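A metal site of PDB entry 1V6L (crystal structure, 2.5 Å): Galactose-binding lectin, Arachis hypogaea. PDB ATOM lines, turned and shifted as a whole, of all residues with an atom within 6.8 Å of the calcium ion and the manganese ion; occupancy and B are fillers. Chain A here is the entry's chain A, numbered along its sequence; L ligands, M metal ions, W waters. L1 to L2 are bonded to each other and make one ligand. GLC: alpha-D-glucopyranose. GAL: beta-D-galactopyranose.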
ATOM      1  N   ASP A  83     -23.145 -10.673   6.125  1.00  0.00           N
ATOM      2  CA  ASP A  83     -23.288 -11.880   6.958  1.00  0.00           C
ATOM      3  C   ASP A  83     -24.764 -12.292   6.838  1.00  0.00           C
ATOM      4  O   ASP A  83     -25.099 -13.453   6.583  1.00  0.00           O
ATOM      5  CB  ASP A  83     -22.879 -11.563   8.406  1.00  0.00           C
ATOM      6  CG  ASP A  83     -21.387 -11.748   8.634  1.00  0.00           C
ATOM      7  OD1 ASP A  83     -20.949 -12.907   8.756  1.00  0.00           O
ATOM      8  OD2 ASP A  83     -20.643 -10.745   8.694  1.00  0.00           O
ATOM      9  N   GLY A 103     -20.180  -9.525  12.229  1.00  0.00           N
ATOM     10  CA  GLY A 103     -19.989 -10.818  11.578  1.00  0.00           C
ATOM     11  C   GLY A 103     -21.076 -11.819  11.923  1.00  0.00           C
ATOM     12  O   GLY A 103     -22.265 -11.497  11.898  1.00  0.00           O
ATOM     13  N   GLY A 104     -20.661 -13.043  12.259  1.00  0.00           N
ATOM     14  CA  GLY A 104     -21.591 -14.096  12.599  1.00  0.00           C
ATOM     15  C   GLY A 104     -22.545 -13.838  13.744  1.00  0.00           C
ATOM     16  O   GLY A 104     -23.592 -14.483  13.832  1.00  0.00           O
ATOM     17  N   THR A 105     -22.217 -12.896  14.632  1.00  0.00           N
ATOM     18  CA  THR A 105     -23.091 -12.608  15.770  1.00  0.00           C
ATOM     19  C   THR A 105     -24.392 -11.967  15.316  1.00  0.00           C
ATOM     20  O   THR A 105     -25.366 -11.933  16.072  1.00  0.00           O
ATOM     21  CB  THR A 105     -22.410 -11.666  16.786  1.00  0.00           C
ATOM     22  OG1 THR A 105     -22.288 -10.349  16.227  1.00  0.00           O
ATOM     23  CG2 THR A 105     -21.041 -12.184  17.144  1.00  0.00           C
ATOM     24  N   LEU A 106     -24.406 -11.455  14.086  1.00  0.00           N
ATOM     25  CA  LEU A 106     -25.596 -10.819  13.523  1.00  0.00           C
ATOM     26  C   LEU A 106     -26.065  -9.596  14.312  1.00  0.00           C
ATOM     27  O   LEU A 106     -27.181  -9.124  14.134  1.00  0.00           O
ATOM     28  CB  LEU A 106     -26.746 -11.826  13.409  1.00  0.00           C
ATOM     29  CG  LEU A 106     -26.461 -13.044  12.513  1.00  0.00           C
ATOM     30  CD1 LEU A 106     -27.688 -13.950  12.481  1.00  0.00           C
ATOM     31  CD2 LEU A 106     -26.122 -12.579  11.110  1.00  0.00           C
ATOM     32  N   GLU A 121     -33.385 -15.921  11.524  1.00  0.00           N
ATOM     33  CA  GLU A 121     -32.230 -15.448  10.769  1.00  0.00           C
ATOM     34  C   GLU A 121     -32.143 -15.896   9.321  1.00  0.00           C
ATOM     35  O   GLU A 121     -32.549 -16.992   8.946  1.00  0.00           O
ATOM     36  CB  GLU A 121     -30.947 -15.866  11.476  1.00  0.00           C
ATOM     37  CG  GLU A 121     -30.745 -17.367  11.528  1.00  0.00           C
ATOM     38  CD  GLU A 121     -29.367 -17.742  11.996  1.00  0.00           C
ATOM     39  OE1 GLU A 121     -28.962 -17.310  13.090  1.00  0.00           O
ATOM     40  OE2 GLU A 121     -28.679 -18.475  11.262  1.00  0.00           O
ATOM     41  N   PHE A 122     -31.572 -15.002   8.518  1.00  0.00           N
ATOM     42  CA  PHE A 122     -31.354 -15.220   7.104  1.00  0.00           C
ATOM     43  C   PHE A 122     -29.855 -15.045   7.009  1.00  0.00           C
ATOM     44  O   PHE A 122     -29.330 -13.979   6.698  1.00  0.00           O
ATOM     45  CB  PHE A 122     -32.143 -14.168   6.343  1.00  0.00           C
ATOM     46  CG  PHE A 122     -33.616 -14.193   6.667  1.00  0.00           C
ATOM     47  CD1 PHE A 122     -34.494 -14.952   5.905  1.00  0.00           C
ATOM     48  CD2 PHE A 122     -34.097 -13.524   7.801  1.00  0.00           C
ATOM     49  CE1 PHE A 122     -35.843 -15.050   6.271  1.00  0.00           C
ATOM     50  CE2 PHE A 122     -35.441 -13.631   8.169  1.00  0.00           C
ATOM     51  CZ  PHE A 122     -36.315 -14.399   7.408  1.00  0.00           C
ATOM     52  N   ASP A 123     -29.175 -16.149   7.327  1.00  0.00           N
ATOM     53  CA  ASP A 123     -27.721 -16.238   7.378  1.00  0.00           C
ATOM     54  C   ASP A 123     -27.078 -16.543   6.036  1.00  0.00           C
ATOM     55  O   ASP A 123     -27.390 -17.554   5.406  1.00  0.00           O
ATOM     56  CB  ASP A 123     -27.364 -17.323   8.372  1.00  0.00           C
ATOM     57  CG  ASP A 123     -26.040 -17.098   8.989  1.00  0.00           C
ATOM     58  OD1 ASP A 123     -25.122 -16.608   8.283  1.00  0.00           O
ATOM     59  OD2 ASP A 123     -25.892 -17.415  10.181  1.00  0.00           O
ATOM     60  N   THR A 124     -26.140 -15.687   5.612  1.00  0.00           N
ATOM     61  CA  THR A 124     -25.482 -15.857   4.329  1.00  0.00           C
ATOM     62  C   THR A 124     -24.021 -16.277   4.380  1.00  0.00           C
ATOM     63  O   THR A 124     -23.368 -16.403   3.341  1.00  0.00           O
ATOM     64  CB  THR A 124     -25.562 -14.565   3.496  1.00  0.00           C
ATOM     65  OG1 THR A 124     -24.836 -13.524   4.168  1.00  0.00           O
ATOM     66  CG2 THR A 124     -27.017 -14.153   3.317  1.00  0.00           C
ATOM     67  N   TYR A 125     -23.497 -16.502   5.573  1.00  0.00           N
ATOM     68  CA  TYR A 125     -22.132 -16.946   5.722  1.00  0.00           C
ATOM     69  C   TYR A 125     -22.096 -18.090   6.729  1.00  0.00           C
ATOM     70  O   TYR A 125     -22.880 -18.100   7.680  1.00  0.00           O
ATOM     71  CB  TYR A 125     -21.218 -15.817   6.189  1.00  0.00           C
ATOM     72  CG  TYR A 125     -19.782 -16.251   6.307  1.00  0.00           C
ATOM     73  CD1 TYR A 125     -19.300 -16.839   7.476  1.00  0.00           C
ATOM     74  CD2 TYR A 125     -18.909 -16.149   5.215  1.00  0.00           C
ATOM     75  CE1 TYR A 125     -17.990 -17.314   7.560  1.00  0.00           C
ATOM     76  CE2 TYR A 125     -17.605 -16.619   5.284  1.00  0.00           C
ATOM     77  CZ  TYR A 125     -17.151 -17.198   6.459  1.00  0.00           C
ATOM     78  OH  TYR A 125     -15.859 -17.671   6.543  1.00  0.00           O
ATOM     79  N   SER A 126     -21.211 -19.052   6.528  1.00  0.00           N
ATOM     80  CA  SER A 126     -21.149 -20.191   7.426  1.00  0.00           C
ATOM     81  C   SER A 126     -20.091 -20.090   8.530  1.00  0.00           C
ATOM     82  O   SER A 126     -18.914 -20.394   8.315  1.00  0.00           O
ATOM     83  CB  SER A 126     -20.928 -21.458   6.583  1.00  0.00           C
ATOM     84  OG  SER A 126     -21.066 -22.625   7.365  1.00  0.00           O
ATOM     85  N   ASN A 127     -20.513 -19.657   9.717  1.00  0.00           N
ATOM     86  CA  ASN A 127     -19.599 -19.537  10.854  1.00  0.00           C
ATOM     87  C   ASN A 127     -19.543 -20.845  11.612  1.00  0.00           C
ATOM     88  O   ASN A 127     -20.466 -21.180  12.353  1.00  0.00           O
ATOM     89  CB  ASN A 127     -20.058 -18.449  11.813  1.00  0.00           C
ATOM     90  CG  ASN A 127     -19.893 -17.064  11.241  1.00  0.00           C
ATOM     91  OD1 ASN A 127     -20.667 -16.647  10.394  1.00  0.00           O
ATOM     92  ND2 ASN A 127     -18.874 -16.343  11.699  1.00  0.00           N
ATOM     93  N   SER A 128     -18.446 -21.581  11.431  1.00  0.00           N
ATOM     94  CA  SER A 128     -18.274 -22.854  12.095  1.00  0.00           C
ATOM     95  C   SER A 128     -18.294 -22.716  13.609  1.00  0.00           C
ATOM     96  O   SER A 128     -18.718 -23.616  14.320  1.00  0.00           O
ATOM     97  CB  SER A 128     -16.978 -23.520  11.646  1.00  0.00           C
ATOM     98  OG  SER A 128     -15.880 -22.652  11.853  1.00  0.00           O
ATOM     99  N   TYR A 130     -20.220 -21.201  15.302  1.00  0.00           N
ATOM    100  CA  TYR A 130     -21.601 -21.214  15.781  1.00  0.00           C
ATOM    101  C   TYR A 130     -22.378 -22.375  15.169  1.00  0.00           C
ATOM    102  O   TYR A 130     -23.607 -22.393  15.180  1.00  0.00           O
ATOM    103  CB  TYR A 130     -22.296 -19.890  15.442  1.00  0.00           C
ATOM    104  CG  TYR A 130     -21.563 -18.670  15.943  1.00  0.00           C
ATOM    105  CD1 TYR A 130     -21.181 -18.552  17.279  1.00  0.00           C
ATOM    106  CD2 TYR A 130     -21.224 -17.629  15.069  1.00  0.00           C
ATOM    107  CE1 TYR A 130     -20.487 -17.419  17.739  1.00  0.00           C
ATOM    108  CE2 TYR A 130     -20.542 -16.505  15.516  1.00  0.00           C
ATOM    109  CZ  TYR A 130     -20.169 -16.416  16.851  1.00  0.00           C
ATOM    110  OH  TYR A 130     -19.454 -15.312  17.280  1.00  0.00           O
ATOM    111  N   ASN A 131     -21.639 -23.342  14.638  1.00  0.00           N
ATOM    112  CA  ASN A 131     -22.223 -24.544  14.040  1.00  0.00           C
ATOM    113  C   ASN A 131     -23.206 -24.310  12.899  1.00  0.00           C
ATOM    114  O   ASN A 131     -24.211 -25.016  12.783  1.00  0.00           O
ATOM    115  CB  ASN A 131     -22.892 -25.394  15.117  1.00  0.00           C
ATOM    116  CG  ASN A 131     -21.923 -25.807  16.214  1.00  0.00           C
ATOM    117  OD1 ASN A 131     -20.855 -26.357  15.939  1.00  0.00           O
ATOM    118  ND2 ASN A 131     -22.291 -25.553  17.463  1.00  0.00           N
ATOM    119  N   ASP A 132     -22.932 -23.323  12.050  1.00  0.00           N
ATOM    120  CA  ASP A 132     -23.805 -23.036  10.920  1.00  0.00           C
ATOM    121  C   ASP A 132     -23.810 -24.170   9.915  1.00  0.00           C
ATOM    122  O   ASP A 132     -22.842 -24.910   9.786  1.00  0.00           O
ATOM    123  CB  ASP A 132     -23.351 -21.796  10.150  1.00  0.00           C
ATOM    124  CG  ASP A 132     -23.770 -20.514  10.797  1.00  0.00           C
ATOM    125  OD1 ASP A 132     -24.846 -20.482  11.418  1.00  0.00           O
ATOM    126  OD2 ASP A 132     -23.025 -19.528  10.644  1.00  0.00           O
ATOM    127  N   PRO A 133     -24.927 -24.325   9.182  1.00  0.00           N
ATOM    128  CA  PRO A 133     -24.959 -25.391   8.186  1.00  0.00           C
ATOM    129  C   PRO A 133     -23.913 -24.938   7.155  1.00  0.00           C
ATOM    130  O   PRO A 133     -23.379 -23.835   7.254  1.00  0.00           O
ATOM    131  CB  PRO A 133     -26.375 -25.296   7.629  1.00  0.00           C
ATOM    132  CG  PRO A 133     -27.163 -24.810   8.822  1.00  0.00           C
ATOM    133  CD  PRO A 133     -26.272 -23.762   9.420  1.00  0.00           C
ATOM    134  N   HIS A 137     -28.853 -20.161   4.862  1.00  0.00           N
ATOM    135  CA  HIS A 137     -29.957 -20.807   5.535  1.00  0.00           C
ATOM    136  C   HIS A 137     -30.838 -19.877   6.347  1.00  0.00           C
ATOM    137  O   HIS A 137     -30.503 -18.718   6.588  1.00  0.00           O
ATOM    138  CB  HIS A 137     -29.399 -21.872   6.473  1.00  0.00           C
ATOM    139  CG  HIS A 137     -28.426 -21.317   7.468  1.00  0.00           C
ATOM    140  ND1 HIS A 137     -27.140 -20.961   7.117  1.00  0.00           N
ATOM    141  CD2 HIS A 137     -28.564 -21.028   8.781  1.00  0.00           C
ATOM    142  CE1 HIS A 137     -26.524 -20.464   8.176  1.00  0.00           C
ATOM    143  NE2 HIS A 137     -27.365 -20.503   9.205  1.00  0.00           N
ATOM    144  N   VAL A 138     -31.967 -20.423   6.763  1.00  0.00           N
ATOM    145  CA  VAL A 138     -32.903 -19.715   7.604  1.00  0.00           C
ATOM    146  C   VAL A 138     -32.860 -20.510   8.903  1.00  0.00           C
ATOM    147  O   VAL A 138     -32.830 -21.749   8.884  1.00  0.00           O
ATOM    148  CB  VAL A 138     -34.310 -19.748   7.022  1.00  0.00           C
ATOM    149  CG1 VAL A 138     -35.282 -19.074   7.970  1.00  0.00           C
ATOM    150  CG2 VAL A 138     -34.325 -19.064   5.665  1.00  0.00           C
ATOM    151  N   GLY A 139     -32.828 -19.824  10.038  1.00  0.00           N
ATOM    152  CA  GLY A 139     -32.776 -20.553  11.295  1.00  0.00           C
ATOM    153  C   GLY A 139     -33.528 -19.867  12.399  1.00  0.00           C
ATOM    154  O   GLY A 139     -33.681 -18.643  12.393  1.00  0.00           O
ATOM    155  N   ASP A 141     -33.558 -18.856  16.150  1.00  0.00           N
ATOM    156  CA  ASP A 141     -32.601 -18.678  17.219  1.00  0.00           C
ATOM    157  C   ASP A 141     -33.270 -18.403  18.545  1.00  0.00           C
ATOM    158  O   ASP A 141     -34.234 -17.636  18.619  1.00  0.00           O
ATOM    159  CB  ASP A 141     -31.632 -17.541  16.905  1.00  0.00           C
ATOM    160  CG  ASP A 141     -30.815 -17.790  15.652  1.00  0.00           C
ATOM    161  OD1 ASP A 141     -30.575 -18.973  15.318  1.00  0.00           O
ATOM    162  OD2 ASP A 141     -30.405 -16.806  15.004  1.00  0.00           O
ATOM    163  N   VAL A 145     -26.970 -17.693  18.367  1.00  0.00           N
ATOM    164  CA  VAL A 145     -26.928 -17.683  16.895  1.00  0.00           C
ATOM    165  C   VAL A 145     -26.632 -19.098  16.455  1.00  0.00           C
ATOM    166  O   VAL A 145     -26.472 -19.387  15.264  1.00  0.00           O
ATOM    167  CB  VAL A 145     -25.854 -16.727  16.357  1.00  0.00           C
ATOM    168  CG1 VAL A 145     -26.297 -15.308  16.574  1.00  0.00           C
ATOM    169  CG2 VAL A 145     -24.526 -17.008  17.044  1.00  0.00           C
ATOM    170  N   ASP A 146     -26.513 -19.980  17.439  1.00  0.00           N
ATOM    171  CA  ASP A 146     -26.306 -21.388  17.178  1.00  0.00           C
ATOM    172  C   ASP A 146     -27.756 -21.856  17.170  1.00  0.00           C
ATOM    173  O   ASP A 146     -28.309 -22.270  18.190  1.00  0.00           O
ATOM    174  CB  ASP A 146     -25.553 -22.053  18.311  1.00  0.00           C
ATOM    175  CG  ASP A 146     -25.235 -23.498  18.013  1.00  0.00           C
ATOM    176  OD1 ASP A 146     -25.919 -24.100  17.147  1.00  0.00           O
ATOM    177  OD2 ASP A 146     -24.315 -24.048  18.654  1.00  0.00           O
ATOM    178  N   SER A 147     -28.374 -21.737  16.006  1.00  0.00           N
ATOM    179  CA  SER A 147     -29.766 -22.086  15.787  1.00  0.00           C
ATOM    180  C   SER A 147     -30.266 -23.399  16.369  1.00  0.00           C
ATOM    181  O   SER A 147     -29.588 -24.423  16.326  1.00  0.00           O
ATOM    182  CB  SER A 147     -30.063 -22.047  14.298  1.00  0.00           C
ATOM    183  OG  SER A 147     -29.704 -20.793  13.757  1.00  0.00           O
ATOM    184  N   THR A 150     -32.370 -25.152  11.645  1.00  0.00           N
ATOM    185  CA  THR A 150     -32.097 -24.424  10.414  1.00  0.00           C
ATOM    186  C   THR A 150     -32.673 -25.189   9.227  1.00  0.00           C
ATOM    187  O   THR A 150     -32.998 -26.368   9.342  1.00  0.00           O
ATOM    188  CB  THR A 150     -30.584 -24.248  10.161  1.00  0.00           C
ATOM    189  OG1 THR A 150     -29.972 -25.539  10.062  1.00  0.00           O
ATOM    190  CG2 THR A 150     -29.933 -23.443  11.276  1.00  0.00           C
HETATM  191  C1  GLC L   1     -10.209 -12.040   8.720  1.00  0.00           C
HETATM  192  C2  GLC L   1     -11.235 -11.399   7.766  1.00  0.00           C
HETATM  193  C3  GLC L   1     -12.624 -11.360   8.423  1.00  0.00           C
HETATM  194  C4  GLC L   1     -13.010 -12.754   8.920  1.00  0.00           C
HETATM  195  C5  GLC L   1     -11.924 -13.286   9.844  1.00  0.00           C
HETATM  196  C6  GLC L   1     -12.213 -14.695  10.350  1.00  0.00           C
HETATM  197  O1  GLC L   1     -10.071 -11.251   9.848  1.00  0.00           O
HETATM  198  O2  GLC L   1     -10.820 -10.087   7.430  1.00  0.00           O
HETATM  199  O3  GLC L   1     -13.584 -10.900   7.490  1.00  0.00           O
HETATM  200  O4  GLC L   1     -14.268 -12.682   9.612  1.00  0.00           O
HETATM  201  O5  GLC L   1     -10.663 -13.335   9.147  1.00  0.00           O
HETATM  202  O6  GLC L   1     -12.506 -15.560   9.273  1.00  0.00           O
HETATM  203  C1  GAL L   2     -15.299 -13.467   9.101  1.00  0.00           C
HETATM  204  C2  GAL L   2     -16.530 -13.328  10.004  1.00  0.00           C
HETATM  205  C3  GAL L   2     -17.715 -14.099   9.398  1.00  0.00           C
HETATM  206  C4  GAL L   2     -17.951 -13.635   7.963  1.00  0.00           C
HETATM  207  C5  GAL L   2     -16.664 -13.772   7.145  1.00  0.00           C
HETATM  208  C6  GAL L   2     -16.829 -13.238   5.746  1.00  0.00           C
HETATM  209  O2  GAL L   2     -16.255 -13.832  11.303  1.00  0.00           O
HETATM  210  O3  GAL L   2     -18.877 -13.888  10.179  1.00  0.00           O
HETATM  211  O4  GAL L   2     -18.362 -12.274   7.968  1.00  0.00           O
HETATM  212  O5  GAL L   2     -15.597 -13.016   7.770  1.00  0.00           O
HETATM  213  O6  GAL L   2     -15.729 -13.598   4.916  1.00  0.00           O
HETATM  214 CA    CA M   1     -23.204 -17.061  10.059  1.00  0.00          CA
HETATM  215 MN    MN M   2     -26.684 -19.337  11.092  1.00  0.00          MN
HETATM  216  O   HOH W   1     -24.026 -16.643  12.518  1.00  0.00           O
HETATM  217  O   HOH W   2     -23.161 -14.492   9.366  1.00  0.00           O
HETATM  218  O   HOH W   3     -26.328 -18.101  13.140  1.00  0.00           O
HETATM  219  O   HOH W   4     -27.635 -21.068  12.133  1.00  0.00           O
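The side-chain carboxylate (OD1) of Asp 83 lies within hydrogen-bond range of an oxygen (O3) of GAL L2.
The backbone NH (N) of Gly 104 sits at hydrogen-bond distance from an oxygen (O3) of GAL L2 (2.9 Å).
ND2 of Asn 127 sits at hydrogen-bond distance from O3 of GAL L2 (2.9 Å).
The backbone NH (N) of Glu 121 sits at hydrogen-bond distance from the backbone carbonyl oxygen (O) of Gly 139, 2.9 Å away.
The side-chain carboxylate (OD2) of Asp 141 sits close to the side-chain carboxylate (OE1) of Glu 121, 2.4 Å away.
Four residues have an atom within 4 Å of the calcium ion: Asp 123, Tyr 125, Asn 127 and Asp 132.
Along chain A the residues within 4 Å of the calcium ion span positions 123 to 132.
Of the 25 residues printed, 4 come within 4 Å of the manganese ion.
The nearest printed residue that does not touch the manganese ion is Val 145 (4.2 Å).
The calcium ion is bound by the side-chain carboxylate (OD2) of Asp 132, the side-chain amide oxygen (OD1) of Asn 127, the backbone carbonyl oxygen (O) of Tyr 125, water W1, the side-chain carboxylate (OD1) of Asp 123, water W2 and the side-chain carboxylate (OD2) of Asp 123.
The calcium ion has seven donor atoms within binding distance.
The manganese ion is bound by OE2 of Glu 121, OD1 of Asp 132, water W4, OD2 of Asp 123, NE2 of His 137 and water W3.
Water W3 bridges the backbone carbonyl oxygen of Val 145 (2.5 Å) and the side-chain carboxylate of Glu 121 (2.8 Å).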
